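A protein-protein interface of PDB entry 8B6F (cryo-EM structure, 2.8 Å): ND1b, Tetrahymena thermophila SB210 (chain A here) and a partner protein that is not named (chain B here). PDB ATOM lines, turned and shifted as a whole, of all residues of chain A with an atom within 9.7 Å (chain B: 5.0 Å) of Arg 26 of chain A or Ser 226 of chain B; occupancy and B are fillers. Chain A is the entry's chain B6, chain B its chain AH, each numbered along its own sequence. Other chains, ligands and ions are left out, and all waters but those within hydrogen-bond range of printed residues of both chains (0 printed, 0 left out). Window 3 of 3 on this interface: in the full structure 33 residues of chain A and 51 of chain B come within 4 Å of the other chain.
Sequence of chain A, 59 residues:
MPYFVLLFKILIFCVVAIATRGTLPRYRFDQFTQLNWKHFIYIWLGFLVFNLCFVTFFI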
ATOM      1  N   THR A  20      -1.360 -15.815  -9.433  1.00  0.00           N
ATOM      2  CA  THR A  20      -1.882 -16.406 -10.660  1.00  0.00           C
ATOM      3  C   THR A  20      -0.925 -17.446 -11.221  1.00  0.00           C
ATOM      4  O   THR A  20      -1.353 -18.511 -11.679  1.00  0.00           O
ATOM      5  CB  THR A  20      -2.155 -15.316 -11.692  1.00  0.00           C
ATOM      6  OG1 THR A  20      -3.074 -14.361 -11.148  1.00  0.00           O
ATOM      7  CG2 THR A  20      -2.756 -15.917 -12.946  1.00  0.00           C
ATOM      8  N   ARG A  21       0.374 -17.160 -11.197  1.00  0.00           N
ATOM      9  CA  ARG A  21       1.344 -18.146 -11.658  1.00  0.00           C
ATOM     10  C   ARG A  21       1.280 -19.405 -10.804  1.00  0.00           C
ATOM     11  O   ARG A  21       1.387 -20.521 -11.324  1.00  0.00           O
ATOM     12  CB  ARG A  21       2.748 -17.547 -11.642  1.00  0.00           C
ATOM     13  CG  ARG A  21       3.809 -18.456 -12.238  1.00  0.00           C
ATOM     14  CD  ARG A  21       4.511 -19.285 -11.179  1.00  0.00           C
ATOM     15  NE  ARG A  21       5.523 -18.510 -10.471  1.00  0.00           N
ATOM     16  CZ  ARG A  21       6.798 -18.431 -10.829  1.00  0.00           C
ATOM     17  NH1 ARG A  21       7.262 -19.069 -11.891  1.00  0.00           N
ATOM     18  NH2 ARG A  21       7.630 -17.691 -10.102  1.00  0.00           N
ATOM     19  N   GLY A  22       1.114 -19.247  -9.491  1.00  0.00           N
ATOM     20  CA  GLY A  22       1.010 -20.398  -8.613  1.00  0.00           C
ATOM     21  C   GLY A  22      -0.285 -21.176  -8.754  1.00  0.00           C
ATOM     22  O   GLY A  22      -0.320 -22.360  -8.406  1.00  0.00           O
ATOM     23  N   THR A  23      -1.351 -20.540  -9.245  1.00  0.00           N
ATOM     24  CA  THR A  23      -2.656 -21.195  -9.323  1.00  0.00           C
ATOM     25  C   THR A  23      -2.905 -21.838 -10.686  1.00  0.00           C
ATOM     26  O   THR A  23      -3.123 -23.050 -10.777  1.00  0.00           O
ATOM     27  CB  THR A  23      -3.784 -20.194  -9.026  1.00  0.00           C
ATOM     28  OG1 THR A  23      -3.820 -19.185 -10.042  1.00  0.00           O
ATOM     29  CG2 THR A  23      -3.616 -19.555  -7.665  1.00  0.00           C
ATOM     30  N   LEU A  24      -2.879 -21.040 -11.749  1.00  0.00           N
ATOM     31  CA  LEU A  24      -3.433 -21.464 -13.025  1.00  0.00           C
ATOM     32  C   LEU A  24      -2.513 -22.430 -13.767  1.00  0.00           C
ATOM     33  O   LEU A  24      -1.303 -22.465 -13.529  1.00  0.00           O
ATOM     34  CB  LEU A  24      -3.709 -20.251 -13.906  1.00  0.00           C
ATOM     35  CG  LEU A  24      -4.887 -19.365 -13.499  1.00  0.00           C
ATOM     36  CD1 LEU A  24      -4.996 -18.186 -14.439  1.00  0.00           C
ATOM     37  CD2 LEU A  24      -6.196 -20.140 -13.478  1.00  0.00           C
ATOM     38  N   PRO A  25      -3.075 -23.238 -14.682  1.00  0.00           N
ATOM     39  CA  PRO A  25      -2.237 -24.065 -15.562  1.00  0.00           C
ATOM     40  C   PRO A  25      -1.604 -23.245 -16.674  1.00  0.00           C
ATOM     41  O   PRO A  25      -1.693 -22.015 -16.665  1.00  0.00           O
ATOM     42  CB  PRO A  25      -3.219 -25.104 -16.127  1.00  0.00           C
ATOM     43  CG  PRO A  25      -4.489 -24.936 -15.356  1.00  0.00           C
ATOM     44  CD  PRO A  25      -4.504 -23.529 -14.874  1.00  0.00           C
ATOM     45  N   ARG A  26      -0.952 -23.911 -17.624  1.00  0.00           N
ATOM     46  CA  ARG A  26      -0.322 -23.256 -18.761  1.00  0.00           C
ATOM     47  C   ARG A  26      -1.050 -23.625 -20.048  1.00  0.00           C
ATOM     48  O   ARG A  26      -1.438 -24.780 -20.244  1.00  0.00           O
ATOM     49  CB  ARG A  26       1.157 -23.638 -18.862  1.00  0.00           C
ATOM     50  CG  ARG A  26       1.855 -23.070 -20.084  1.00  0.00           C
ATOM     51  CD  ARG A  26       3.367 -23.193 -19.982  1.00  0.00           C
ATOM     52  NE  ARG A  26       3.798 -24.542 -19.632  1.00  0.00           N
ATOM     53  CZ  ARG A  26       4.140 -24.938 -18.411  1.00  0.00           C
ATOM     54  NH1 ARG A  26       4.113 -24.109 -17.380  1.00  0.00           N
ATOM     55  NH2 ARG A  26       4.519 -26.197 -18.222  1.00  0.00           N
ATOM     56  N   TYR A  27      -1.235 -22.634 -20.917  1.00  0.00           N
ATOM     57  CA  TYR A  27      -1.908 -22.824 -22.193  1.00  0.00           C
ATOM     58  C   TYR A  27      -0.961 -23.448 -23.217  1.00  0.00           C
ATOM     59  O   TYR A  27       0.250 -23.546 -23.013  1.00  0.00           O
ATOM     60  CB  TYR A  27      -2.424 -21.487 -22.732  1.00  0.00           C
ATOM     61  CG  TYR A  27      -3.923 -21.310 -22.674  1.00  0.00           C
ATOM     62  CD1 TYR A  27      -4.775 -22.194 -23.323  1.00  0.00           C
ATOM     63  CD2 TYR A  27      -4.484 -20.232 -22.005  1.00  0.00           C
ATOM     64  CE1 TYR A  27      -6.144 -22.023 -23.281  1.00  0.00           C
ATOM     65  CE2 TYR A  27      -5.850 -20.054 -21.957  1.00  0.00           C
ATOM     66  CZ  TYR A  27      -6.674 -20.952 -22.597  1.00  0.00           C
ATOM     67  OH  TYR A  27      -8.038 -20.776 -22.554  1.00  0.00           O
ATOM     68  N   ARG A  28      -1.536 -23.871 -24.339  1.00  0.00           N
ATOM     69  CA  ARG A  28      -0.777 -24.200 -25.537  1.00  0.00           C
ATOM     70  C   ARG A  28      -0.752 -22.990 -26.460  1.00  0.00           C
ATOM     71  O   ARG A  28      -1.710 -22.216 -26.520  1.00  0.00           O
ATOM     72  CB  ARG A  28      -1.378 -25.397 -26.276  1.00  0.00           C
ATOM     73  CG  ARG A  28      -1.298 -26.713 -25.530  1.00  0.00           C
ATOM     74  CD  ARG A  28      -1.279 -27.887 -26.500  1.00  0.00           C
ATOM     75  NE  ARG A  28      -2.345 -27.820 -27.494  1.00  0.00           N
ATOM     76  CZ  ARG A  28      -3.530 -28.403 -27.379  1.00  0.00           C
ATOM     77  NH1 ARG A  28      -3.859 -29.098 -26.302  1.00  0.00           N
ATOM     78  NH2 ARG A  28      -4.407 -28.289 -28.370  1.00  0.00           N
ATOM     79  N   PHE A  29       0.357 -22.826 -27.184  1.00  0.00           N
ATOM     80  CA  PHE A  29       0.482 -21.664 -28.057  1.00  0.00           C
ATOM     81  C   PHE A  29      -0.583 -21.680 -29.147  1.00  0.00           C
ATOM     82  O   PHE A  29      -1.181 -20.642 -29.453  1.00  0.00           O
ATOM     83  CB  PHE A  29       1.888 -21.588 -28.662  1.00  0.00           C
ATOM     84  CG  PHE A  29       2.338 -22.847 -29.346  1.00  0.00           C
ATOM     85  CD1 PHE A  29       2.039 -23.075 -30.678  1.00  0.00           C
ATOM     86  CD2 PHE A  29       3.099 -23.782 -28.666  1.00  0.00           C
ATOM     87  CE1 PHE A  29       2.465 -24.224 -31.310  1.00  0.00           C
ATOM     88  CE2 PHE A  29       3.527 -24.932 -29.292  1.00  0.00           C
ATOM     89  CZ  PHE A  29       3.210 -25.154 -30.616  1.00  0.00           C
ATOM     90  N   ASP A  30      -0.828 -22.843 -29.755  1.00  0.00           N
ATOM     91  CA  ASP A  30      -1.857 -22.925 -30.786  1.00  0.00           C
ATOM     92  C   ASP A  30      -3.240 -22.653 -30.207  1.00  0.00           C
ATOM     93  O   ASP A  30      -4.047 -21.942 -30.816  1.00  0.00           O
ATOM     94  CB  ASP A  30      -1.822 -24.293 -31.460  1.00  0.00           C
ATOM     95  CG  ASP A  30      -2.129 -25.417 -30.500  1.00  0.00           C
ATOM     96  OD1 ASP A  30      -1.628 -25.370 -29.358  1.00  0.00           O
ATOM     97  OD2 ASP A  30      -2.879 -26.340 -30.877  1.00  0.00           O
ATOM     98  N   GLN A  31      -3.537 -23.218 -29.034  1.00  0.00           N
ATOM     99  CA  GLN A  31      -4.836 -22.989 -28.411  1.00  0.00           C
ATOM    100  C   GLN A  31      -5.065 -21.508 -28.144  1.00  0.00           C
ATOM    101  O   GLN A  31      -6.119 -20.960 -28.483  1.00  0.00           O
ATOM    102  CB  GLN A  31      -4.943 -23.783 -27.110  1.00  0.00           C
ATOM    103  CG  GLN A  31      -5.146 -25.267 -27.308  1.00  0.00           C
ATOM    104  CD  GLN A  31      -5.310 -25.997 -25.995  1.00  0.00           C
ATOM    105  OE1 GLN A  31      -4.847 -25.535 -24.954  1.00  0.00           O
ATOM    106  NE2 GLN A  31      -5.983 -27.140 -26.035  1.00  0.00           N
ATOM    107  N   PHE A  32      -4.084 -20.841 -27.538  1.00  0.00           N
ATOM    108  CA  PHE A  32      -4.259 -19.428 -27.225  1.00  0.00           C
ATOM    109  C   PHE A  32      -4.354 -18.589 -28.489  1.00  0.00           C
ATOM    110  O   PHE A  32      -5.138 -17.636 -28.551  1.00  0.00           O
ATOM    111  CB  PHE A  32      -3.117 -18.922 -26.351  1.00  0.00           C
ATOM    112  CG  PHE A  32      -3.127 -17.437 -26.178  1.00  0.00           C
ATOM    113  CD1 PHE A  32      -4.183 -16.811 -25.540  1.00  0.00           C
ATOM    114  CD2 PHE A  32      -2.096 -16.663 -26.680  1.00  0.00           C
ATOM    115  CE1 PHE A  32      -4.203 -15.440 -25.391  1.00  0.00           C
ATOM    116  CE2 PHE A  32      -2.110 -15.293 -26.534  1.00  0.00           C
ATOM    117  CZ  PHE A  32      -3.166 -14.681 -25.889  1.00  0.00           C
ATOM    118  N   PRO B 218      -1.173 -18.282 -17.649  1.00  0.00           N
ATOM    119  CA  PRO B 218      -0.964 -19.462 -18.491  1.00  0.00           C
ATOM    120  C   PRO B 218      -0.166 -19.156 -19.751  1.00  0.00           C
ATOM    121  O   PRO B 218      -0.332 -19.824 -20.765  1.00  0.00           O
ATOM    122  CB  PRO B 218      -2.403 -19.901 -18.833  1.00  0.00           C
ATOM    123  CG  PRO B 218      -3.337 -18.820 -18.279  1.00  0.00           C
ATOM    124  CD  PRO B 218      -2.468 -17.653 -17.935  1.00  0.00           C
ATOM    125  N   ASP B 220       3.386 -18.785 -19.894  1.00  0.00           N
ATOM    126  CA  ASP B 220       4.811 -19.062 -19.724  1.00  0.00           C
ATOM    127  C   ASP B 220       5.281 -20.121 -20.718  1.00  0.00           C
ATOM    128  O   ASP B 220       5.898 -21.120 -20.356  1.00  0.00           O
ATOM    129  CB  ASP B 220       5.077 -19.495 -18.287  1.00  0.00           C
ATOM    130  CG  ASP B 220       6.553 -19.675 -17.993  1.00  0.00           C
ATOM    131  OD1 ASP B 220       7.305 -18.684 -18.093  1.00  0.00           O
ATOM    132  OD2 ASP B 220       6.958 -20.807 -17.654  1.00  0.00           O
ATOM    133  N   LEU B 221       4.987 -19.892 -21.999  1.00  0.00           N
ATOM    134  CA  LEU B 221       5.296 -20.883 -23.023  1.00  0.00           C
ATOM    135  C   LEU B 221       6.776 -20.888 -23.380  1.00  0.00           C
ATOM    136  O   LEU B 221       7.363 -21.955 -23.591  1.00  0.00           O
ATOM    137  CB  LEU B 221       4.449 -20.631 -24.270  1.00  0.00           C
ATOM    138  CG  LEU B 221       2.959 -20.380 -24.018  1.00  0.00           C
ATOM    139  CD1 LEU B 221       2.225 -20.188 -25.331  1.00  0.00           C
ATOM    140  CD2 LEU B 221       2.336 -21.513 -23.217  1.00  0.00           C
ATOM    141  N   ALA B 224       8.602 -22.514 -20.515  1.00  0.00           N
ATOM    142  CA  ALA B 224       7.948 -23.716 -20.014  1.00  0.00           C
ATOM    143  C   ALA B 224       8.982 -24.747 -19.590  1.00  0.00           C
ATOM    144  O   ALA B 224       9.754 -25.244 -20.415  1.00  0.00           O
ATOM    145  CB  ALA B 224       7.028 -24.296 -21.089  1.00  0.00           C
ATOM    146  N   GLU B 225       8.989 -25.070 -18.299  1.00  0.00           N
ATOM    147  CA  GLU B 225       9.990 -25.960 -17.729  1.00  0.00           C
ATOM    148  C   GLU B 225       9.599 -27.430 -17.796  1.00  0.00           C
ATOM    149  O   GLU B 225      10.464 -28.290 -17.604  1.00  0.00           O
ATOM    150  CB  GLU B 225      10.269 -25.570 -16.271  1.00  0.00           C
ATOM    151  CG  GLU B 225       9.041 -25.565 -15.368  1.00  0.00           C
ATOM    152  CD  GLU B 225       9.329 -24.976 -14.001  1.00  0.00           C
ATOM    153  OE1 GLU B 225      10.516 -24.755 -13.687  1.00  0.00           O
ATOM    154  OE2 GLU B 225       8.368 -24.726 -13.243  1.00  0.00           O
ATOM    155  N   SER B 226       8.333 -27.743 -18.064  1.00  0.00           N
ATOM    156  CA  SER B 226       7.893 -29.123 -18.231  1.00  0.00           C
ATOM    157  C   SER B 226       7.865 -29.536 -19.696  1.00  0.00           C
ATOM    158  O   SER B 226       8.396 -30.590 -20.054  1.00  0.00           O
ATOM    159  CB  SER B 226       6.507 -29.318 -17.607  1.00  0.00           C
ATOM    160  OG  SER B 226       5.536 -28.515 -18.255  1.00  0.00           O
ATOM    161  N   GLU B 227       7.247 -28.722 -20.553  1.00  0.00           N
ATOM    162  CA  GLU B 227       7.236 -29.020 -21.980  1.00  0.00           C
ATOM    163  C   GLU B 227       8.645 -28.974 -22.559  1.00  0.00           C
ATOM    164  O   GLU B 227       9.010 -29.809 -23.395  1.00  0.00           O
ATOM    165  CB  GLU B 227       6.320 -28.034 -22.705  1.00  0.00           C
ATOM    166  CG  GLU B 227       4.887 -28.035 -22.185  1.00  0.00           C
ATOM    167  CD  GLU B 227       4.089 -26.839 -22.662  1.00  0.00           C
ATOM    168  OE1 GLU B 227       4.592 -26.091 -23.524  1.00  0.00           O
ATOM    169  OE2 GLU B 227       2.956 -26.645 -22.173  1.00  0.00           O
ATOM    170  N   LEU B 228       9.445 -28.007 -22.126  1.00  0.00           N
ATOM    171  CA  LEU B 228      10.838 -27.882 -22.517  1.00  0.00           C
ATOM    172  C   LEU B 228      11.705 -27.949 -21.269  1.00  0.00           C
ATOM    173  O   LEU B 228      11.232 -27.732 -20.151  1.00  0.00           O
ATOM    174  CB  LEU B 228      11.083 -26.569 -23.271  1.00  0.00           C
ATOM    175  CG  LEU B 228      10.158 -26.329 -24.467  1.00  0.00           C
ATOM    176  CD1 LEU B 228      10.369 -24.943 -25.037  1.00  0.00           C
ATOM    177  CD2 LEU B 228      10.376 -27.380 -25.540  1.00  0.00           C
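Among the printed residues, pairs that only touch across the chains: Tyr 27 of chain A with Leu 221 of chain B (2.9 Å), Pro 25 of chain A with Pro 218 of chain B (3.1 Å), Arg 26 of chain A with Asp 220 of chain B (3.3 Å), Arg 26 of chain A with Leu 221 of chain B (3.5 Å), Arg 26 of chain A with Ala 224 of chain B (3.6 Å), Phe 29 of chain A with Leu 221 of chain B (3.6 Å) and Arg 26 of chain A with Pro 218 of chain B (3.9 Å).
Printed residues of chain B within 4 Å of Arg 26 of chain A: Pro 218, Asp 220, Leu 221, Ala 224, Ser 226 and Glu 227. Of the printed residues of chain A, Ser 226 of chain B touches Arg 26 (2.5 Å). Of the printed residues of chain A, Glu 227 of chain B touches Arg 26 (3.4 Å). Of the printed residues of chain B, Tyr 27 of chain A touches Pro 218 (3.0 Å) and Leu 221 (2.9 Å). Of the printed residues of chain A, Pro 218 of chain B touches Pro 25, Arg 26 and Tyr 27. Gln 31 of chain A touches none of the printed residues of chain B. Leu 228 of chain B touches none of the printed residues of chain A. The nearest printed residue of chain B that does not touch Tyr 27 of chain A is Glu 227 of chain B (4.2 Å).
OG of Ser 226 of chain B sits at hydrogen-bond distance from NH2 of Arg 26 of chain A, at 2.5 Å. NE of Arg 26 of chain A lies within salt-bridge range of OE2 of Glu 227 of chain B (3.4 Å). O of Pro 218 of chain B sits at hydrogen-bond distance from N of Tyr 27 of chain A.
Printed residues of chain B that touch a printed residue of chain A: Pro 218, Asp 220, Leu 221, Ala 224, Ser 226 and Glu 227. Of the 13 printed residues of chain A, 4 touch a printed residue of chain B. Printed residues of chain A that touch a printed residue of chain B: Pro 25, Arg 26, Tyr 27 and Phe 29. Hydrophobic or aromatic side chains of chain A that line the printed part of chain B: Tyr 27 and Phe 29. Along chain A the printed residues that touch a printed residue of chain B span positions 25 to 29. Among the printed residues, Asp or Glu carboxylates within 4 Å of a Lys or Arg side-chain nitrogen of the other chain: Arg 26 of chain A with Glu 227 of chain B (3.4 Å).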
